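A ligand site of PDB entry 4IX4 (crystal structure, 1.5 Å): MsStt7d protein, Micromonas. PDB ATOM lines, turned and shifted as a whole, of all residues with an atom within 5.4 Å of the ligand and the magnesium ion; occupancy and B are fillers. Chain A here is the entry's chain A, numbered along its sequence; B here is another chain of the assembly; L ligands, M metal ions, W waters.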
ATOM      1  N   LEU A  28     -22.910  16.404 -12.141  1.00  0.00           N
ATOM      2  CA  LEU A  28     -22.460  15.218 -12.866  1.00  0.00           C
ATOM      3  C   LEU A  28     -21.040  15.327 -13.383  1.00  0.00           C
ATOM      4  O   LEU A  28     -20.403  14.314 -13.693  1.00  0.00           O
ATOM      5  CB  LEU A  28     -23.367  14.956 -14.060  1.00  0.00           C
ATOM      6  CG  LEU A  28     -24.877  14.869 -13.866  1.00  0.00           C
ATOM      7  CD1 LEU A  28     -25.545  14.555 -15.197  1.00  0.00           C
ATOM      8  CD2 LEU A  28     -25.233  13.820 -12.828  1.00  0.00           C
ATOM      9  N   GLY A  29     -20.532  16.555 -13.494  1.00  0.00           N
ATOM     10  CA  GLY A  29     -19.262  16.771 -14.166  1.00  0.00           C
ATOM     11  C   GLY A  29     -18.049  16.829 -13.259  1.00  0.00           C
ATOM     12  O   GLY A  29     -18.139  16.646 -12.043  1.00  0.00           O
ATOM     13  N   SER A  30     -16.891  17.085 -13.868  1.00  0.00           N
ATOM     14  CA  SER A  30     -15.694  17.398 -13.088  1.00  0.00           C
ATOM     15  C   SER A  30     -15.732  18.863 -12.669  1.00  0.00           C
ATOM     16  O   SER A  30     -14.962  19.286 -11.803  1.00  0.00           O
ATOM     17  CB  SER A  30     -14.408  17.062 -13.869  1.00  0.00           C
ATOM     18  OG  SER A  30     -14.315  17.793 -15.088  1.00  0.00           O
ATOM     19  N   GLY A  31     -16.625  19.627 -13.276  1.00  0.00           N
ATOM     20  CA  GLY A  31     -16.901  20.997 -12.885  1.00  0.00           C
ATOM     21  C   GLY A  31     -15.792  22.005 -13.068  1.00  0.00           C
ATOM     22  O   GLY A  31     -15.374  22.672 -12.122  1.00  0.00           O
ATOM     23  N   ASN A  32     -15.306  22.112 -14.306  1.00  0.00           N
ATOM     24  CA  ASN A  32     -14.238  23.038 -14.652  1.00  0.00           C
ATOM     25  C   ASN A  32     -14.746  24.453 -14.888  1.00  0.00           C
ATOM     26  O   ASN A  32     -14.511  25.345 -14.076  1.00  0.00           O
ATOM     27  CB  ASN A  32     -13.480  22.544 -15.884  1.00  0.00           C
ATOM     28  CG  ASN A  32     -12.404  21.522 -15.540  1.00  0.00           C
ATOM     29  OD1 ASN A  32     -11.873  21.516 -14.434  1.00  0.00           O
ATOM     30  ND2 ASN A  32     -12.094  20.650 -16.486  1.00  0.00           N
ATOM     31  N   GLY A  34     -18.156  24.928 -16.049  1.00  0.00           N
ATOM     32  CA  GLY A  34     -19.592  24.892 -15.899  1.00  0.00           C
ATOM     33  C   GLY A  34     -20.020  23.787 -14.967  1.00  0.00           C
ATOM     34  O   GLY A  34     -19.213  22.964 -14.539  1.00  0.00           O
ATOM     35  N   VAL A  36     -23.042  20.743 -14.430  1.00  0.00           N
ATOM     36  CA  VAL A  36     -24.020  19.950 -15.170  1.00  0.00           C
ATOM     37  C   VAL A  36     -24.973  19.232 -14.227  1.00  0.00           C
ATOM     38  O   VAL A  36     -24.535  18.622 -13.247  1.00  0.00           O
ATOM     39  CB  VAL A  36     -23.299  18.935 -16.085  1.00  0.00           C
ATOM     40  CG1 VAL A  36     -24.302  18.065 -16.813  1.00  0.00           C
ATOM     41  CG2 VAL A  36     -22.402  19.666 -17.061  1.00  0.00           C
ATOM     42  N   VAL A  48     -30.289  16.998 -19.715  1.00  0.00           N
ATOM     43  CA  VAL A  48     -29.132  17.427 -18.949  1.00  0.00           C
ATOM     44  C   VAL A  48     -28.945  18.922 -19.168  1.00  0.00           C
ATOM     45  O   VAL A  48     -29.126  19.418 -20.275  1.00  0.00           O
ATOM     46  CB  VAL A  48     -27.866  16.653 -19.340  1.00  0.00           C
ATOM     47  CG1 VAL A  48     -28.056  15.168 -19.077  1.00  0.00           C
ATOM     48  CG2 VAL A  48     -27.529  16.904 -20.801  1.00  0.00           C
ATOM     49  N   LYS A  50     -26.589  22.577 -18.366  1.00  0.00           N
ATOM     50  CA  LYS A  50     -25.266  23.099 -18.016  1.00  0.00           C
ATOM     51  C   LYS A  50     -25.314  24.610 -17.852  1.00  0.00           C
ATOM     52  O   LYS A  50     -25.881  25.318 -18.686  1.00  0.00           O
ATOM     53  CB  LYS A  50     -24.225  22.729 -19.092  1.00  0.00           C
ATOM     54  CG  LYS A  50     -22.814  23.219 -18.771  1.00  0.00           C
ATOM     55  CD  LYS A  50     -21.813  22.889 -19.890  1.00  0.00           C
ATOM     56  CE  LYS A  50     -21.535  21.378 -20.001  1.00  0.00           C
ATOM     57  NZ  LYS A  50     -20.499  21.004 -21.035  1.00  0.00           N
ATOM     58  N   GLU A  66     -19.490  27.345 -26.486  1.00  0.00           N
ATOM     59  CA  GLU A  66     -20.040  25.994 -26.491  1.00  0.00           C
ATOM     60  C   GLU A  66     -21.454  25.990 -27.086  1.00  0.00           C
ATOM     61  O   GLU A  66     -21.819  25.084 -27.842  1.00  0.00           O
ATOM     62  CB  GLU A  66     -20.026  25.395 -25.077  1.00  0.00           C
ATOM     63  CG  GLU A  66     -20.698  24.044 -24.974  1.00  0.00           C
ATOM     64  CD  GLU A  66     -20.480  23.349 -23.633  1.00  0.00           C
ATOM     65  OE1 GLU A  66     -19.780  23.904 -22.753  1.00  0.00           O
ATOM     66  OE2 GLU A  66     -21.024  22.249 -23.455  1.00  0.00           O
ATOM     67  N   ALA A  82     -24.557  14.437 -28.371  1.00  0.00           N
ATOM     68  CA  ALA A  82     -25.844  14.429 -27.673  1.00  0.00           C
ATOM     69  C   ALA A  82     -26.781  15.443 -28.324  1.00  0.00           C
ATOM     70  O   ALA A  82     -26.363  16.537 -28.708  1.00  0.00           O
ATOM     71  CB  ALA A  82     -25.661  14.772 -26.212  1.00  0.00           C
ATOM     72  N   TRP A 111     -29.599  19.512 -23.224  1.00  0.00           N
ATOM     73  CA  TRP A 111     -29.515  18.401 -24.160  1.00  0.00           C
ATOM     74  C   TRP A 111     -30.415  17.263 -23.703  1.00  0.00           C
ATOM     75  O   TRP A 111     -30.752  17.167 -22.520  1.00  0.00           O
ATOM     76  CB  TRP A 111     -28.101  17.830 -24.208  1.00  0.00           C
ATOM     77  CG  TRP A 111     -27.013  18.787 -24.605  1.00  0.00           C
ATOM     78  CD1 TRP A 111     -26.481  18.975 -25.859  1.00  0.00           C
ATOM     79  CD2 TRP A 111     -26.296  19.673 -23.735  1.00  0.00           C
ATOM     80  NE1 TRP A 111     -25.493  19.934 -25.817  1.00  0.00           N
ATOM     81  CE2 TRP A 111     -25.352  20.360 -24.524  1.00  0.00           C
ATOM     82  CE3 TRP A 111     -26.354  19.928 -22.359  1.00  0.00           C
ATOM     83  CZ2 TRP A 111     -24.482  21.309 -23.981  1.00  0.00           C
ATOM     84  CZ3 TRP A 111     -25.485  20.864 -21.831  1.00  0.00           C
ATOM     85  CH2 TRP A 111     -24.552  21.534 -22.645  1.00  0.00           C
ATOM     86  N   ALA A 112     -30.760  16.381 -24.634  1.00  0.00           N
ATOM     87  CA  ALA A 112     -31.380  15.113 -24.267  1.00  0.00           C
ATOM     88  C   ALA A 112     -30.413  14.334 -23.383  1.00  0.00           C
ATOM     89  O   ALA A 112     -29.210  14.330 -23.619  1.00  0.00           O
ATOM     90  CB  ALA A 112     -31.696  14.292 -25.517  1.00  0.00           C
ATOM     91  N   ASN A 113     -30.946  13.662 -22.370  1.00  0.00           N
ATOM     92  CA  ASN A 113     -30.128  12.720 -21.617  1.00  0.00           C
ATOM     93  C   ASN A 113     -29.962  11.466 -22.480  1.00  0.00           C
ATOM     94  O   ASN A 113     -30.918  10.751 -22.745  1.00  0.00           O
ATOM     95  CB  ASN A 113     -30.764  12.400 -20.252  1.00  0.00           C
ATOM     96  CG  ASN A 113     -29.909  11.472 -19.423  1.00  0.00           C
ATOM     97  OD1 ASN A 113     -29.154  10.670 -19.971  1.00  0.00           O
ATOM     98  ND2 ASN A 113     -30.022  11.568 -18.096  1.00  0.00           N
ATOM     99  N   GLU A 114     -28.728  11.238 -22.935  1.00  0.00           N
ATOM    100  CA  GLU A 114     -28.457  10.181 -23.910  1.00  0.00           C
ATOM    101  C   GLU A 114     -28.169   8.839 -23.246  1.00  0.00           C
ATOM    102  O   GLU A 114     -28.093   7.815 -23.917  1.00  0.00           O
ATOM    103  CB  GLU A 114     -27.271  10.567 -24.803  1.00  0.00           C
ATOM    104  CG  GLU A 114     -27.530  11.792 -25.682  1.00  0.00           C
ATOM    105  CD  GLU A 114     -28.504  11.526 -26.806  1.00  0.00           C
ATOM    106  OE1 GLU A 114     -28.870  10.357 -27.031  1.00  0.00           O
ATOM    107  OE2 GLU A 114     -28.888  12.488 -27.481  1.00  0.00           O
ATOM    108  N   GLY A 115     -28.011   8.848 -21.928  1.00  0.00           N
ATOM    109  CA  GLY A 115     -27.739   7.612 -21.220  1.00  0.00           C
ATOM    110  C   GLY A 115     -27.031   7.843 -19.914  1.00  0.00           C
ATOM    111  O   GLY A 115     -26.392   8.863 -19.725  1.00  0.00           O
ATOM    112  N   THR A 118     -21.025   6.749 -19.245  1.00  0.00           N
ATOM    113  CA  THR A 118     -20.003   7.091 -20.210  1.00  0.00           C
ATOM    114  C   THR A 118     -19.190   5.849 -20.538  1.00  0.00           C
ATOM    115  O   THR A 118     -19.205   4.863 -19.786  1.00  0.00           O
ATOM    116  CB  THR A 118     -19.035   8.172 -19.700  1.00  0.00           C
ATOM    117  OG1 THR A 118     -18.243   7.652 -18.631  1.00  0.00           O
ATOM    118  CG2 THR A 118     -19.796   9.420 -19.252  1.00  0.00           C
ATOM    119  N   ASP A 168     -11.610  17.419 -27.218  1.00  0.00           N
ATOM    120  CA  ASP A 168     -11.730  16.755 -25.924  1.00  0.00           C
ATOM    121  C   ASP A 168     -12.264  15.353 -26.083  1.00  0.00           C
ATOM    122  O   ASP A 168     -13.096  14.907 -25.287  1.00  0.00           O
ATOM    123  CB  ASP A 168     -12.592  17.564 -24.965  1.00  0.00           C
ATOM    124  CG  ASP A 168     -12.311  17.235 -23.510  1.00  0.00           C
ATOM    125  OD1 ASP A 168     -13.077  17.677 -22.634  1.00  0.00           O
ATOM    126  OD2 ASP A 168     -11.318  16.516 -23.253  1.00  0.00           O
ATOM    127  N   LYS A 170     -12.354  11.557 -25.615  1.00  0.00           N
ATOM    128  CA  LYS A 170     -11.897  10.608 -24.594  1.00  0.00           C
ATOM    129  C   LYS A 170     -13.082   9.762 -24.153  1.00  0.00           C
ATOM    130  O   LYS A 170     -14.220  10.133 -24.381  1.00  0.00           O
ATOM    131  CB  LYS A 170     -11.279  11.327 -23.393  1.00  0.00           C
ATOM    132  CG  LYS A 170     -12.193  12.336 -22.720  1.00  0.00           C
ATOM    133  CD  LYS A 170     -11.430  13.153 -21.694  1.00  0.00           C
ATOM    134  CE  LYS A 170     -12.337  14.186 -21.054  1.00  0.00           C
ATOM    135  NZ  LYS A 170     -11.604  15.373 -20.566  1.00  0.00           N
ATOM    136  N   ALA A 172     -14.502   9.425 -21.352  1.00  0.00           N
ATOM    137  CA  ALA A 172     -15.420  10.166 -20.477  1.00  0.00           C
ATOM    138  C   ALA A 172     -16.397  11.077 -21.235  1.00  0.00           C
ATOM    139  O   ALA A 172     -17.402  11.501 -20.679  1.00  0.00           O
ATOM    140  CB  ALA A 172     -14.646  10.983 -19.464  1.00  0.00           C
ATOM    141  N   ASN A 173     -16.089  11.375 -22.501  1.00  0.00           N
ATOM    142  CA  ASN A 173     -16.938  12.220 -23.317  1.00  0.00           C
ATOM    143  C   ASN A 173     -17.658  11.447 -24.405  1.00  0.00           C
ATOM    144  O   ASN A 173     -18.017  12.002 -25.461  1.00  0.00           O
ATOM    145  CB  ASN A 173     -16.162  13.389 -23.919  1.00  0.00           C
ATOM    146  CG  ASN A 173     -15.924  14.517 -22.912  1.00  0.00           C
ATOM    147  OD1 ASN A 173     -16.662  14.647 -21.928  1.00  0.00           O
ATOM    148  ND2 ASN A 173     -14.905  15.331 -23.152  1.00  0.00           N
ATOM    149  N   ILE A 175     -20.958   8.653 -24.710  1.00  0.00           N
ATOM    150  CA  ILE A 175     -22.045   7.948 -24.066  1.00  0.00           C
ATOM    151  C   ILE A 175     -22.637   6.910 -25.039  1.00  0.00           C
ATOM    152  O   ILE A 175     -22.885   7.229 -26.205  1.00  0.00           O
ATOM    153  CB  ILE A 175     -23.160   8.928 -23.603  1.00  0.00           C
ATOM    154  CG1 ILE A 175     -22.604   9.873 -22.515  1.00  0.00           C
ATOM    155  CG2 ILE A 175     -24.396   8.170 -23.102  1.00  0.00           C
ATOM    156  CD1 ILE A 175     -23.639  10.835 -21.953  1.00  0.00           C
ATOM    157  N   ILE A 187     -20.093  13.932 -26.186  1.00  0.00           N
ATOM    158  CA  ILE A 187     -20.607  15.060 -25.423  1.00  0.00           C
ATOM    159  C   ILE A 187     -19.492  16.079 -25.204  1.00  0.00           C
ATOM    160  O   ILE A 187     -18.322  15.799 -25.500  1.00  0.00           O
ATOM    161  CB  ILE A 187     -21.191  14.637 -24.055  1.00  0.00           C
ATOM    162  CG1 ILE A 187     -20.143  13.880 -23.232  1.00  0.00           C
ATOM    163  CG2 ILE A 187     -22.477  13.834 -24.221  1.00  0.00           C
ATOM    164  CD1 ILE A 187     -20.528  13.703 -21.775  1.00  0.00           C
ATOM    165  N   ASP A 188     -19.863  17.222 -24.653  1.00  0.00           N
ATOM    166  CA  ASP A 188     -18.884  18.216 -24.215  1.00  0.00           C
ATOM    167  C   ASP A 188     -18.143  18.892 -25.371  1.00  0.00           C
ATOM    168  O   ASP A 188     -16.993  18.563 -25.651  1.00  0.00           O
ATOM    169  CB  ASP A 188     -17.887  17.588 -23.249  1.00  0.00           C
ATOM    170  CG  ASP A 188     -17.185  18.621 -22.380  1.00  0.00           C
ATOM    171  OD1 ASP A 188     -17.403  19.829 -22.606  1.00  0.00           O
ATOM    172  OD2 ASP A 188     -16.419  18.219 -21.480  1.00  0.00           O
ATOM    173  N   ASP B  55      -8.362  15.322 -15.467  1.00  0.00           N
ATOM    174  CA  ASP B  55      -8.674  15.899 -16.772  1.00  0.00           C
ATOM    175  C   ASP B  55      -8.136  17.312 -16.969  1.00  0.00           C
ATOM    176  O   ASP B  55      -8.374  17.932 -18.006  1.00  0.00           O
ATOM    177  CB  ASP B  55     -10.188  15.845 -17.039  1.00  0.00           C
ATOM    178  CG  ASP B  55     -11.004  16.616 -16.001  1.00  0.00           C
ATOM    179  OD1 ASP B  55     -10.596  16.689 -14.835  1.00  0.00           O
ATOM    180  OD2 ASP B  55     -12.073  17.129 -16.372  1.00  0.00           O
HETATM  181  P1  LIG L   1     -17.612  18.435 -17.978  1.00  0.00           P
HETATM  182  O1  LIG L   1     -17.998  18.188 -16.543  1.00  0.00           O
HETATM  183  O2  LIG L   1     -16.968  19.774 -18.249  1.00  0.00           O
HETATM  184  O3  LIG L   1     -16.865  17.270 -18.570  1.00  0.00           O
HETATM  185  P2  LIG L   1     -19.774  17.439 -19.664  1.00  0.00           P
HETATM  186  O4  LIG L   1     -18.791  16.346 -20.016  1.00  0.00           O
HETATM  187  O5  LIG L   1     -20.457  18.223 -20.746  1.00  0.00           O
HETATM  188  O6  LIG L   1     -19.040  18.561 -18.740  1.00  0.00           O
HETATM  189  O7  LIG L   1     -20.881  16.786 -18.689  1.00  0.00           O
HETATM  190  C1  LIG L   1     -20.546  16.342 -17.375  1.00  0.00           C
HETATM  191  C2  LIG L   1     -21.143  14.951 -17.167  1.00  0.00           C
HETATM  192  O8  LIG L   1     -22.565  14.949 -17.326  1.00  0.00           O
HETATM  193  C3  LIG L   1     -20.627  13.932 -18.184  1.00  0.00           C
HETATM  194  O9  LIG L   1     -19.431  13.309 -17.731  1.00  0.00           O
HETATM  195  C4  LIG L   1     -21.735  12.916 -18.252  1.00  0.00           C
HETATM  196  O10 LIG L   1     -21.633  12.021 -17.142  1.00  0.00           O
HETATM  197  C5  LIG L   1     -22.966  13.759 -18.007  1.00  0.00           C
HETATM  198  N1  LIG L   1     -23.587  14.217 -19.279  1.00  0.00           N
HETATM  199  C6  LIG L   1     -23.271  15.321 -19.987  1.00  0.00           C
HETATM  200  N2  LIG L   1     -24.061  15.432 -21.075  1.00  0.00           N
HETATM  201  C7  LIG L   1     -24.915  14.394 -21.061  1.00  0.00           C
HETATM  202  C8  LIG L   1     -26.023  13.915 -21.905  1.00  0.00           C
HETATM  203  N3  LIG L   1     -26.396  14.589 -23.029  1.00  0.00           N
HETATM  204  N4  LIG L   1     -26.651  12.783 -21.519  1.00  0.00           N
HETATM  205  C9  LIG L   1     -26.309  12.096 -20.421  1.00  0.00           C
HETATM  206  N5  LIG L   1     -25.315  12.488 -19.604  1.00  0.00           N
HETATM  207  C10 LIG L   1     -24.598  13.600 -19.876  1.00  0.00           C
HETATM  208 MG    MG M   1     -16.609  16.301 -20.345  1.00  0.00          MG
HETATM  209  O   HOH W   1     -14.916  19.403 -19.810  1.00  0.00           O
HETATM  210  O   HOH W   2     -18.941  20.086 -14.850  1.00  0.00           O
HETATM  211  O   HOH W   3     -25.073  10.312 -17.770  1.00  0.00           O
HETATM  212  O   HOH W   4     -15.345  15.961 -16.685  1.00  0.00           O
HETATM  213  O   HOH W   5     -15.001  19.952 -16.322  1.00  0.00           O
HETATM  214  O   HOH W   6     -24.325  17.242 -23.141  1.00  0.00           O
HETATM  215  O   HOH W   7     -17.759  15.392 -16.213  1.00  0.00           O
HETATM  216  O   HOH W   8     -14.410  15.973 -20.049  1.00  0.00           O
HETATM  217  O   HOH W   9     -17.116  14.081 -19.323  1.00  0.00           O
HETATM  218  O   HOH W  10     -22.813   9.903 -16.490  1.00  0.00           O
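The backbone carbonyl oxygen of Trp 111 lies within hydrogen-bond range of the backbone NH of Val 48 (2.8 Å). NZ of Lys 50 is in salt-bridge range of OE2 of Glu 66, 2.8 Å away. The backbone NH (N) of Gly 115 is in hydrogen-bond range of the side-chain amide oxygen (OD1) of Asn 113 (2.9 Å). The side-chain amino group (NZ) of Lys 50 is in salt-bridge range of the side-chain carboxylate (OD1) of Asp 188 (3.7 Å). The backbone NH (N) of Leu 28 sits at hydrogen-bond distance from the backbone carbonyl oxygen (O) of Val 36, at 3.0 Å. The backbone carbonyl oxygen (O) of Asn 173 lies within hydrogen-bond range of the backbone NH (N) of Ile 187 (2.9 Å). OD2 of Asp 55 of chain B lies within hydrogen-bond range of OG of Ser 30, 2.7 Å away. ND2 of Asn 173 sits at hydrogen-bond distance from O of Asp 168 (2.8 Å).
Within 4 Å of the magnesium ion: Asn 173 and Asp 188.
Water W9 lies within hydrogen-bond range of an oxygen (O9) of the ligand (2.9 Å) and the backbone carbonyl oxygen (O) of Ala 172 (2.9 Å). Water W2 lies within hydrogen-bond range of O1 of the ligand (2.7 Å), N of Gly 31 (2.8 Å) and O of Gly 34 (2.9 Å). Water W4 lies within hydrogen-bond range of the side-chain hydroxyl of Ser 30 (2.6 Å), an oxygen (O1) of the ligand (3.5 Å) and the side-chain carboxylate of Asp 55 of chain B (3.5 Å). Water W5 lies within hydrogen-bond range of the side-chain hydroxyl (OG) of Ser 30 (2.6 Å), an oxygen (O2) of the ligand (2.8 Å), the backbone NH (N) of Asn 32 (3.0 Å) and the backbone NH (N) of Gly 31 (3.5 Å). Water W7 bridges an oxygen (O1) of the ligand (2.8 Å) and the backbone NH of Ser 30 (3.0 Å). Water W3 bridges O of Gly 115 (2.8 Å) and N5 of the ligand (2.9 Å).
Merely in contact with the ligand: Gly 29 (3.0 Å), Asn 113 (3.2 Å), Ala 82 (3.3 Å), Gly 115 (3.3 Å), Ile 175 (3.3 Å), Leu 28 (3.4 Å), Val 48 (3.4 Å), Ile 187 (3.6 Å), Val 36 (3.6 Å), Thr 118 (3.8 Å), Gly 31 (3.8 Å) and Trp 111 (3.8 Å). Hydrophobic or aromatic side chains within 4 Å of the ligand: Leu 28, Val 36, Val 48, Ala 82, Trp 111, Ile 175 and Ile 187. Within 4 Å of the ligand: Leu 28, Gly 29, Ser 30, Gly 31, Val 36, Val 48, Lys 50, Ala 82, Trp 111, Ala 112, Asn 113, Glu 114, Gly 115, Thr 118, Asn 173, Ile 175, Ile 187 and Asp 188.
The magnesium ion is bound by an oxygen (O3) of the ligand (2.0 Å), an oxygen (O4) of the ligand (2.2 Å), the side-chain carboxylate (OD2) of Asp 188 (2.2 Å), water W8 (2.2 Å), the side-chain amide oxygen (OD1) of Asn 173 (2.3 Å) and water W9 (2.5 Å).
N of Ser 30 lies within hydrogen-bond range of O1 of the ligand (3.1 Å). O5 of the ligand is in salt-bridge range of NZ of Lys 50 (2.8 Å). The backbone carbonyl oxygen of Ala 112 sits at hydrogen-bond distance from a nitrogen (N3) of the ligand, at 2.9 Å. A nitrogen (N4) of the ligand sits at hydrogen-bond distance from the backbone NH of Glu 114 (3.0 Å).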
